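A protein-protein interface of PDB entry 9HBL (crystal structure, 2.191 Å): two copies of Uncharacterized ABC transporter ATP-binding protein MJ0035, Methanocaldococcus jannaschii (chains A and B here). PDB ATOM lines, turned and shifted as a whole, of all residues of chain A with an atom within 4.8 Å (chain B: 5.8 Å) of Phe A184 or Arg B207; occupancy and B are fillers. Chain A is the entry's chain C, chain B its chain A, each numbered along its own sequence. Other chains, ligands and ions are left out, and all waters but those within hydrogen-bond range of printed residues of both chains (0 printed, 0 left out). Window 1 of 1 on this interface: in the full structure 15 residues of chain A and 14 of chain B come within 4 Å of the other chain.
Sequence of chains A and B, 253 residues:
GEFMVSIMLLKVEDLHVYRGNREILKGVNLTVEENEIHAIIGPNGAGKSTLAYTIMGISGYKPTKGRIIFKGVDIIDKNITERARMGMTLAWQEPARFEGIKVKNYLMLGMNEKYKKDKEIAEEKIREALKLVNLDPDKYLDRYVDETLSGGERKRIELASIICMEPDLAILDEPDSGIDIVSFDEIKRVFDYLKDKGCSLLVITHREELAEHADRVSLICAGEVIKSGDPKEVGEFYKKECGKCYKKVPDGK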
ATOM      1  N   ASP A 176      11.462   9.123  -6.274  1.00  0.00           N
ATOM      2  CA  ASP A 176      11.124   8.715  -7.644  1.00  0.00           C
ATOM      3  C   ASP A 176      12.005   7.567  -8.201  1.00  0.00           C
ATOM      4  O   ASP A 176      11.821   7.150  -9.348  1.00  0.00           O
ATOM      5  CB  ASP A 176      11.122   9.929  -8.592  1.00  0.00           C
ATOM      6  CG  ASP A 176      12.496  10.370  -9.062  1.00  0.00           C
ATOM      7  OD1 ASP A 176      13.480  10.189  -8.289  1.00  0.00           O
ATOM      8  OD2 ASP A 176      12.594  10.895 -10.208  1.00  0.00           O
ATOM      9  N   ILE A 181       8.480   4.781 -12.323  1.00  0.00           N
ATOM     10  CA  ILE A 181       7.739   6.016 -12.548  1.00  0.00           C
ATOM     11  C   ILE A 181       7.427   6.252 -14.017  1.00  0.00           C
ATOM     12  O   ILE A 181       8.305   6.189 -14.869  1.00  0.00           O
ATOM     13  CB  ILE A 181       8.472   7.212 -11.881  1.00  0.00           C
ATOM     14  CG1 ILE A 181       7.526   8.393 -11.616  1.00  0.00           C
ATOM     15  CG2 ILE A 181       9.705   7.622 -12.659  1.00  0.00           C
ATOM     16  CD1 ILE A 181       8.147   9.536 -10.836  1.00  0.00           C
ATOM     17  N   VAL A 182       6.143   6.464 -14.311  1.00  0.00           N
ATOM     18  CA  VAL A 182       5.648   6.731 -15.658  1.00  0.00           C
ATOM     19  C   VAL A 182       6.041   8.153 -16.065  1.00  0.00           C
ATOM     20  O   VAL A 182       6.582   8.368 -17.152  1.00  0.00           O
ATOM     21  CB  VAL A 182       4.120   6.514 -15.698  1.00  0.00           C
ATOM     22  CG1 VAL A 182       3.518   7.005 -17.007  1.00  0.00           C
ATOM     23  CG2 VAL A 182       3.775   5.054 -15.444  1.00  0.00           C
ATOM     24  N   SER A 183       5.821   9.111 -15.161  1.00  0.00           N
ATOM     25  CA  SER A 183       6.139  10.527 -15.356  1.00  0.00           C
ATOM     26  C   SER A 183       6.145  11.268 -13.998  1.00  0.00           C
ATOM     27  O   SER A 183       5.665  10.716 -13.006  1.00  0.00           O
ATOM     28  CB  SER A 183       5.130  11.175 -16.306  1.00  0.00           C
ATOM     29  OG  SER A 183       3.825  11.199 -15.747  1.00  0.00           O
ATOM     30  N   PHE A 184       6.655  12.525 -13.950  1.00  0.00           N
ATOM     31  CA  PHE A 184       6.642  13.296 -12.695  1.00  0.00           C
ATOM     32  C   PHE A 184       5.246  13.659 -12.213  1.00  0.00           C
ATOM     33  O   PHE A 184       5.095  14.073 -11.071  1.00  0.00           O
ATOM     34  CB  PHE A 184       7.525  14.541 -12.758  1.00  0.00           C
ATOM     35  CG  PHE A 184       8.987  14.212 -12.917  1.00  0.00           C
ATOM     36  CD1 PHE A 184       9.667  13.514 -11.933  1.00  0.00           C
ATOM     37  CD2 PHE A 184       9.675  14.580 -14.060  1.00  0.00           C
ATOM     38  CE1 PHE A 184      11.009  13.208 -12.081  1.00  0.00           C
ATOM     39  CE2 PHE A 184      11.015  14.264 -14.211  1.00  0.00           C
ATOM     40  CZ  PHE A 184      11.674  13.580 -13.220  1.00  0.00           C
ATOM     41  N   ASP A 185       4.226  13.498 -13.072  1.00  0.00           N
ATOM     42  CA  ASP A 185       2.836  13.719 -12.694  1.00  0.00           C
ATOM     43  C   ASP A 185       2.356  12.665 -11.678  1.00  0.00           C
ATOM     44  O   ASP A 185       1.459  12.945 -10.886  1.00  0.00           O
ATOM     45  CB  ASP A 185       1.943  13.726 -13.949  1.00  0.00           C
ATOM     46  CG  ASP A 185       2.308  14.815 -14.936  1.00  0.00           C
ATOM     47  OD1 ASP A 185       2.970  15.801 -14.523  1.00  0.00           O
ATOM     48  OD2 ASP A 185       1.931  14.693 -16.118  1.00  0.00           O
ATOM     49  N   GLU A 186       2.964  11.466 -11.697  1.00  0.00           N
ATOM     50  CA  GLU A 186       2.650  10.388 -10.780  1.00  0.00           C
ATOM     51  C   GLU A 186       3.113  10.757  -9.361  1.00  0.00           C
ATOM     52  O   GLU A 186       2.336  10.643  -8.406  1.00  0.00           O
ATOM     53  CB  GLU A 186       3.345   9.104 -11.253  1.00  0.00           C
ATOM     54  CG  GLU A 186       2.401   7.934 -11.438  1.00  0.00           C
ATOM     55  CD  GLU A 186       3.097   6.613 -11.687  1.00  0.00           C
ATOM     56  OE1 GLU A 186       4.288   6.623 -12.076  1.00  0.00           O
ATOM     57  OE2 GLU A 186       2.448   5.561 -11.486  1.00  0.00           O
ATOM     58  N   ILE A 187       4.364  11.244  -9.235  1.00  0.00           N
ATOM     59  CA  ILE A 187       4.926  11.612  -7.941  1.00  0.00           C
ATOM     60  C   ILE A 187       4.350  12.937  -7.433  1.00  0.00           C
ATOM     61  O   ILE A 187       4.108  13.073  -6.231  1.00  0.00           O
ATOM     62  CB  ILE A 187       6.481  11.577  -7.980  1.00  0.00           C
ATOM     63  CG1 ILE A 187       7.078  11.274  -6.598  1.00  0.00           C
ATOM     64  CG2 ILE A 187       7.096  12.818  -8.603  1.00  0.00           C
ATOM     65  CD1 ILE A 187       6.718   9.948  -6.064  1.00  0.00           C
ATOM     66  N   LYS A 188       4.059  13.885  -8.357  1.00  0.00           N
ATOM     67  CA  LYS A 188       3.475  15.186  -8.014  1.00  0.00           C
ATOM     68  C   LYS A 188       2.066  15.037  -7.448  1.00  0.00           C
ATOM     69  O   LYS A 188       1.705  15.768  -6.536  1.00  0.00           O
ATOM     70  CB  LYS A 188       3.513  16.175  -9.199  1.00  0.00           C
ATOM     71  CG  LYS A 188       2.461  15.936 -10.270  1.00  0.00           C
ATOM     72  CD  LYS A 188       2.019  17.229 -10.944  1.00  0.00           C
ATOM     73  CE  LYS A 188       0.889  17.905 -10.210  1.00  0.00           C
ATOM     74  NZ  LYS A 188       0.734  19.328 -10.614  1.00  0.00           N
ATOM     75  N   ARG A 207      18.401  14.058  -8.851  1.00  0.00           N
ATOM     76  CA  ARG A 207      17.748  14.389 -10.111  1.00  0.00           C
ATOM     77  C   ARG A 207      17.145  15.770 -10.070  1.00  0.00           C
ATOM     78  O   ARG A 207      16.149  15.987  -9.399  1.00  0.00           O
ATOM     79  CB  ARG A 207      16.671  13.347 -10.453  1.00  0.00           C
ATOM     80  CG  ARG A 207      16.325  13.329 -11.931  1.00  0.00           C
ATOM     81  CD  ARG A 207      15.227  12.339 -12.255  1.00  0.00           C
ATOM     82  NE  ARG A 207      15.681  10.959 -12.114  1.00  0.00           N
ATOM     83  CZ  ARG A 207      16.047  10.179 -13.128  1.00  0.00           C
ATOM     84  NH1 ARG A 207      16.040  10.646 -14.374  1.00  0.00           N
ATOM     85  NH2 ARG A 207      16.444   8.935 -12.902  1.00  0.00           N
ATOM     86  N   GLU A 209      15.422  17.408 -12.322  1.00  0.00           N
ATOM     87  CA  GLU A 209      14.064  17.442 -12.866  1.00  0.00           C
ATOM     88  C   GLU A 209      13.022  17.232 -11.776  1.00  0.00           C
ATOM     89  O   GLU A 209      11.963  17.848 -11.830  1.00  0.00           O
ATOM     90  CB  GLU A 209      13.891  16.403 -13.987  1.00  0.00           C
ATOM     91  CG  GLU A 209      14.599  16.752 -15.275  1.00  0.00           C
ATOM     92  CD  GLU A 209      16.063  16.368 -15.356  1.00  0.00           C
ATOM     93  OE1 GLU A 209      16.608  15.867 -14.346  1.00  0.00           O
ATOM     94  OE2 GLU A 209      16.667  16.560 -16.438  1.00  0.00           O
ATOM     95  N   LEU A 210      13.334  16.383 -10.780  1.00  0.00           N
ATOM     96  CA  LEU A 210      12.444  16.106  -9.656  1.00  0.00           C
ATOM     97  C   LEU A 210      12.337  17.314  -8.686  1.00  0.00           C
ATOM     98  O   LEU A 210      11.233  17.680  -8.257  1.00  0.00           O
ATOM     99  CB  LEU A 210      12.913  14.839  -8.911  1.00  0.00           C
ATOM    100  CG  LEU A 210      12.006  14.372  -7.769  1.00  0.00           C
ATOM    101  CD1 LEU A 210      10.636  13.953  -8.283  1.00  0.00           C
ATOM    102  CD2 LEU A 210      12.650  13.249  -6.978  1.00  0.00           C
ATOM    103  N   HIS A 213       9.861  20.575  -9.155  1.00  0.00           N
ATOM    104  CA  HIS A 213       8.464  20.533  -8.707  1.00  0.00           C
ATOM    105  C   HIS A 213       8.274  20.955  -7.221  1.00  0.00           C
ATOM    106  O   HIS A 213       7.136  21.081  -6.759  1.00  0.00           O
ATOM    107  CB  HIS A 213       7.853  19.132  -8.969  1.00  0.00           C
ATOM    108  CG  HIS A 213       8.060  18.628 -10.369  1.00  0.00           C
ATOM    109  ND1 HIS A 213       7.128  18.860 -11.371  1.00  0.00           N
ATOM    110  CD2 HIS A 213       9.097  17.936 -10.894  1.00  0.00           C
ATOM    111  CE1 HIS A 213       7.634  18.317 -12.468  1.00  0.00           C
ATOM    112  NE2 HIS A 213       8.822  17.756 -12.233  1.00  0.00           N
ATOM    113  N   ILE B  41       8.716   2.470 -24.554  1.00  0.00           N
ATOM    114  CA  ILE B  41       8.084   2.790 -23.282  1.00  0.00           C
ATOM    115  C   ILE B  41       6.981   1.807 -22.958  1.00  0.00           C
ATOM    116  O   ILE B  41       6.411   1.190 -23.853  1.00  0.00           O
ATOM    117  CB  ILE B  41       7.585   4.250 -23.193  1.00  0.00           C
ATOM    118  CG1 ILE B  41       6.599   4.567 -24.330  1.00  0.00           C
ATOM    119  CG2 ILE B  41       8.746   5.214 -23.140  1.00  0.00           C
ATOM    120  CD1 ILE B  41       5.947   5.914 -24.220  1.00  0.00           C
ATOM    121  N   GLU B 174      16.991   0.502 -19.412  1.00  0.00           N
ATOM    122  CA  GLU B 174      16.902   1.552 -18.390  1.00  0.00           C
ATOM    123  C   GLU B 174      18.239   2.267 -18.177  1.00  0.00           C
ATOM    124  O   GLU B 174      18.767   2.253 -17.072  1.00  0.00           O
ATOM    125  CB  GLU B 174      16.365   0.981 -17.049  1.00  0.00           C
ATOM    126  CG  GLU B 174      15.145   0.099 -17.189  1.00  0.00           C
ATOM    127  CD  GLU B 174      13.866   0.847 -17.491  1.00  0.00           C
ATOM    128  OE1 GLU B 174      12.862   0.166 -17.796  1.00  0.00           O
ATOM    129  OE2 GLU B 174      13.857   2.098 -17.424  1.00  0.00           O
ATOM    130  N   ASP B 176      19.140   5.351 -17.656  1.00  0.00           N
ATOM    131  CA  ASP B 176      19.200   6.455 -16.690  1.00  0.00           C
ATOM    132  C   ASP B 176      18.918   6.033 -15.231  1.00  0.00           C
ATOM    133  O   ASP B 176      18.938   6.880 -14.338  1.00  0.00           O
ATOM    134  CB  ASP B 176      18.283   7.618 -17.124  1.00  0.00           C
ATOM    135  CG  ASP B 176      16.814   7.428 -16.802  1.00  0.00           C
ATOM    136  OD1 ASP B 176      16.353   6.264 -16.792  1.00  0.00           O
ATOM    137  OD2 ASP B 176      16.123   8.446 -16.562  1.00  0.00           O
ATOM    138  N   PHE B 184      18.881  14.976 -17.534  1.00  0.00           N
ATOM    139  CA  PHE B 184      18.885  14.272 -18.824  1.00  0.00           C
ATOM    140  C   PHE B 184      19.983  14.743 -19.764  1.00  0.00           C
ATOM    141  O   PHE B 184      20.291  14.045 -20.715  1.00  0.00           O
ATOM    142  CB  PHE B 184      17.532  14.338 -19.528  1.00  0.00           C
ATOM    143  CG  PHE B 184      16.481  13.518 -18.829  1.00  0.00           C
ATOM    144  CD1 PHE B 184      16.666  12.163 -18.613  1.00  0.00           C
ATOM    145  CD2 PHE B 184      15.315  14.106 -18.368  1.00  0.00           C
ATOM    146  CE1 PHE B 184      15.702  11.413 -17.963  1.00  0.00           C
ATOM    147  CE2 PHE B 184      14.360  13.354 -17.702  1.00  0.00           C
ATOM    148  CZ  PHE B 184      14.557  12.011 -17.511  1.00  0.00           C
ATOM    149  N   THR B 205      12.762   1.862 -21.665  1.00  0.00           N
ATOM    150  CA  THR B 205      12.497   2.691 -20.482  1.00  0.00           C
ATOM    151  C   THR B 205      11.025   2.724 -20.074  1.00  0.00           C
ATOM    152  O   THR B 205      10.150   2.489 -20.895  1.00  0.00           O
ATOM    153  CB  THR B 205      13.015   4.148 -20.695  1.00  0.00           C
ATOM    154  OG1 THR B 205      12.987   4.846 -19.455  1.00  0.00           O
ATOM    155  CG2 THR B 205      12.218   4.924 -21.754  1.00  0.00           C
ATOM    156  N   HIS B 206      10.760   3.026 -18.806  1.00  0.00           N
ATOM    157  CA  HIS B 206       9.411   3.251 -18.274  1.00  0.00           C
ATOM    158  C   HIS B 206       9.162   4.776 -18.068  1.00  0.00           C
ATOM    159  O   HIS B 206       8.012   5.187 -17.898  1.00  0.00           O
ATOM    160  CB  HIS B 206       9.207   2.529 -16.932  1.00  0.00           C
ATOM    161  CG  HIS B 206      10.267   2.840 -15.920  1.00  0.00           C
ATOM    162  ND1 HIS B 206      10.437   4.124 -15.416  1.00  0.00           N
ATOM    163  CD2 HIS B 206      11.188   2.024 -15.358  1.00  0.00           C
ATOM    164  CE1 HIS B 206      11.456   4.047 -14.575  1.00  0.00           C
ATOM    165  NE2 HIS B 206      11.941   2.805 -14.509  1.00  0.00           N
ATOM    166  N   ARG B 207      10.250   5.597 -18.016  1.00  0.00           N
ATOM    167  CA  ARG B 207      10.207   7.035 -17.786  1.00  0.00           C
ATOM    168  C   ARG B 207       9.983   7.777 -19.083  1.00  0.00           C
ATOM    169  O   ARG B 207      10.885   7.848 -19.919  1.00  0.00           O
ATOM    170  CB  ARG B 207      11.510   7.505 -17.130  1.00  0.00           C
ATOM    171  CG  ARG B 207      11.375   8.846 -16.434  1.00  0.00           C
ATOM    172  CD  ARG B 207      12.672   9.308 -15.809  1.00  0.00           C
ATOM    173  NE  ARG B 207      13.045   8.486 -14.659  1.00  0.00           N
ATOM    174  CZ  ARG B 207      12.837   8.823 -13.389  1.00  0.00           C
ATOM    175  NH1 ARG B 207      12.240   9.971 -13.087  1.00  0.00           N
ATOM    176  NH2 ARG B 207      13.210   8.007 -12.410  1.00  0.00           N
ATOM    177  N   GLU B 208       8.771   8.321 -19.257  1.00  0.00           N
ATOM    178  CA  GLU B 208       8.343   9.061 -20.453  1.00  0.00           C
ATOM    179  C   GLU B 208       9.268  10.257 -20.752  1.00  0.00           C
ATOM    180  O   GLU B 208       9.518  10.575 -21.913  1.00  0.00           O
ATOM    181  CB  GLU B 208       6.876   9.518 -20.269  1.00  0.00           C
ATOM    182  CG  GLU B 208       6.187  10.038 -21.516  1.00  0.00           C
ATOM    183  CD  GLU B 208       6.362  11.521 -21.780  1.00  0.00           C
ATOM    184  OE1 GLU B 208       6.539  12.288 -20.804  1.00  0.00           O
ATOM    185  OE2 GLU B 208       6.329  11.914 -22.970  1.00  0.00           O
ATOM    186  N   GLU B 209       9.786  10.900 -19.704  1.00  0.00           N
ATOM    187  CA  GLU B 209      10.668  12.054 -19.837  1.00  0.00           C
ATOM    188  C   GLU B 209      11.947  11.717 -20.596  1.00  0.00           C
ATOM    189  O   GLU B 209      12.410  12.537 -21.382  1.00  0.00           O
ATOM    190  CB  GLU B 209      10.981  12.661 -18.454  1.00  0.00           C
ATOM    191  CG  GLU B 209       9.844  13.453 -17.840  1.00  0.00           C
ATOM    192  CD  GLU B 209       8.780  12.648 -17.116  1.00  0.00           C
ATOM    193  OE1 GLU B 209       8.899  11.402 -17.071  1.00  0.00           O
ATOM    194  OE2 GLU B 209       7.826  13.270 -16.589  1.00  0.00           O
ATOM    195  N   LEU B 210      12.493  10.500 -20.392  1.00  0.00           N
ATOM    196  CA  LEU B 210      13.701  10.019 -21.080  1.00  0.00           C
ATOM    197  C   LEU B 210      13.442   9.720 -22.566  1.00  0.00           C
ATOM    198  O   LEU B 210      14.295   9.989 -23.418  1.00  0.00           O
ATOM    199  CB  LEU B 210      14.264   8.765 -20.382  1.00  0.00           C
ATOM    200  CG  LEU B 210      15.511   8.133 -21.012  1.00  0.00           C
ATOM    201  CD1 LEU B 210      16.667   9.105 -21.018  1.00  0.00           C
ATOM    202  CD2 LEU B 210      15.908   6.857 -20.282  1.00  0.00           C
ATOM    203  N   ALA B 211      12.261   9.185 -22.874  1.00  0.00           N
ATOM    204  CA  ALA B 211      11.893   8.850 -24.245  1.00  0.00           C
ATOM    205  C   ALA B 211      11.720  10.056 -25.173  1.00  0.00           C
ATOM    206  O   ALA B 211      11.931   9.920 -26.373  1.00  0.00           O
ATOM    207  CB  ALA B 211      10.632   8.005 -24.250  1.00  0.00           C
ATOM    208  N   TYR B 238       0.772   7.564 -23.600  1.00  0.00           N
ATOM    209  CA  TYR B 238       1.212   6.634 -22.551  1.00  0.00           C
ATOM    210  C   TYR B 238       0.819   7.123 -21.151  1.00  0.00           C
ATOM    211  O   TYR B 238       0.266   6.348 -20.369  1.00  0.00           O
ATOM    212  CB  TYR B 238       2.740   6.405 -22.661  1.00  0.00           C
ATOM    213  CG  TYR B 238       3.433   5.777 -21.463  1.00  0.00           C
ATOM    214  CD1 TYR B 238       3.016   4.556 -20.952  1.00  0.00           C
ATOM    215  CD2 TYR B 238       4.572   6.350 -20.916  1.00  0.00           C
ATOM    216  CE1 TYR B 238       3.679   3.949 -19.895  1.00  0.00           C
ATOM    217  CE2 TYR B 238       5.257   5.743 -19.872  1.00  0.00           C
ATOM    218  CZ  TYR B 238       4.800   4.547 -19.356  1.00  0.00           C
ATOM    219  OH  TYR B 238       5.447   3.958 -18.298  1.00  0.00           O
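The guanidinium group of Arg A207 is in salt-bridge range of the side-chain carboxylate of Asp B176 (3.1 Å).
The backbone NH of Phe B184 lies within hydrogen-bond range of the side-chain carboxylate of Glu A209 (2.9 Å).
O of Ile A181 lies within hydrogen-bond range of ND1 of His B206.
The side-chain carboxylate (OD2) of Asp A176 is in salt-bridge range of the guanidinium group (NH1) of Arg B207 (3.0 Å).
N of Glu B208 is in hydrogen-bond range of O of Val A182, 3.0 Å away.
The side-chain carboxylate (OE2) of Glu B209 sits at hydrogen-bond distance from the backbone NH (N) of Phe A184.
The guanidinium group (NH2) of Arg A207 sits close to the guanidinium group (NH2) of Arg B207 (3.4 Å).
Among the printed residues, 15 pairs touch across the chains.
Among the printed residues, Asp or Glu carboxylates within 4 Å of a Lys or Arg side-chain nitrogen of the other chain: Asp A176 with Arg B207 (3.0 Å) and Arg A207 with Asp B176 (3.1 Å).
OD2 of Asp B176 is in salt-bridge range of NE of Arg B207, at 3.6 Å.
OG1 of Thr B205 sits at hydrogen-bond distance from N of Arg B207 (3.2 Å).
OH of Tyr B238 lies within hydrogen-bond range of O of His B206, 2.9 Å away.
NE of Arg A207 is in salt-bridge range of OD2 of Asp A176, 3.6 Å away.
OE1 of Glu A186 lies within hydrogen-bond range of N of Val A182 (2.9 Å).
The backbone carbonyl oxygen (O) of Glu A209 sits close to a ring nitrogen (NE2) of His A213 (3.2 Å).
Arg B207 touches Ile A181 (CZ to CG2, 3.4 Å).
O of Val A182 touches O of His B206, at 3.6 Å.
Arg B207 touches Val A182 (CA to O, 3.9 Å).
Glu B209 touches Val A182.
Val A182 touches Tyr B238.
CA of Ser A183 touches OE1 of Glu B209 (3.4 Å).
CE1 of Phe A184 touches NH1 of Arg B207, 3.6 Å away.
Arg A207 touches Phe B184 (NH1 to CE1, 3.7 Å).
Asp A176 touches Arg B207, and with the chains exchanged Arg A207 touches Asp B176.
Phe A184 touches Arg B207, and with the chains exchanged Arg A207 touches Phe B184.
Phe A184 touches Glu B209, and with the chains exchanged Glu A209 touches Phe B184.
Arg A207 touches its own counterpart, Arg B207.
5 positions are printed for both chains.
Of the 15 pairs that touch across the chains among the printed residues, 7 have their exchanged pair printed and touching as well.
Of chain B, only Arg B207 (3.6 Å) and Glu B209 (3.0 Å) come within 4 Å of Phe A184.
Of the printed residues of chain A, Arg B207 touches Asp A176, Ile A181, Val A182, Phe A184 and Arg A207.
Of the printed residues of chain B, Ile A181 touches His B206 (3.0 Å) and Arg B207 (3.4 Å).
Of the printed residues of chain B, Arg A207 touches Asp B176 (3.1 Å), Phe B184 (3.7 Å) and Arg B207 (3.4 Å).
Of the printed residues of chain A, Glu B209 touches Val A182, Ser A183 and Phe A184.
Of the printed residues of chain A, Phe B184 touches Arg A207 (3.7 Å) and Glu A209 (2.9 Å).
Of the printed residues of chain B, Val A182 touches His B206, Arg B207, Glu B208, Glu B209 and Tyr B238.
Ala B211 touches none of the printed residues of chain A.
Leu A210 touches none of the printed residues of chain B.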
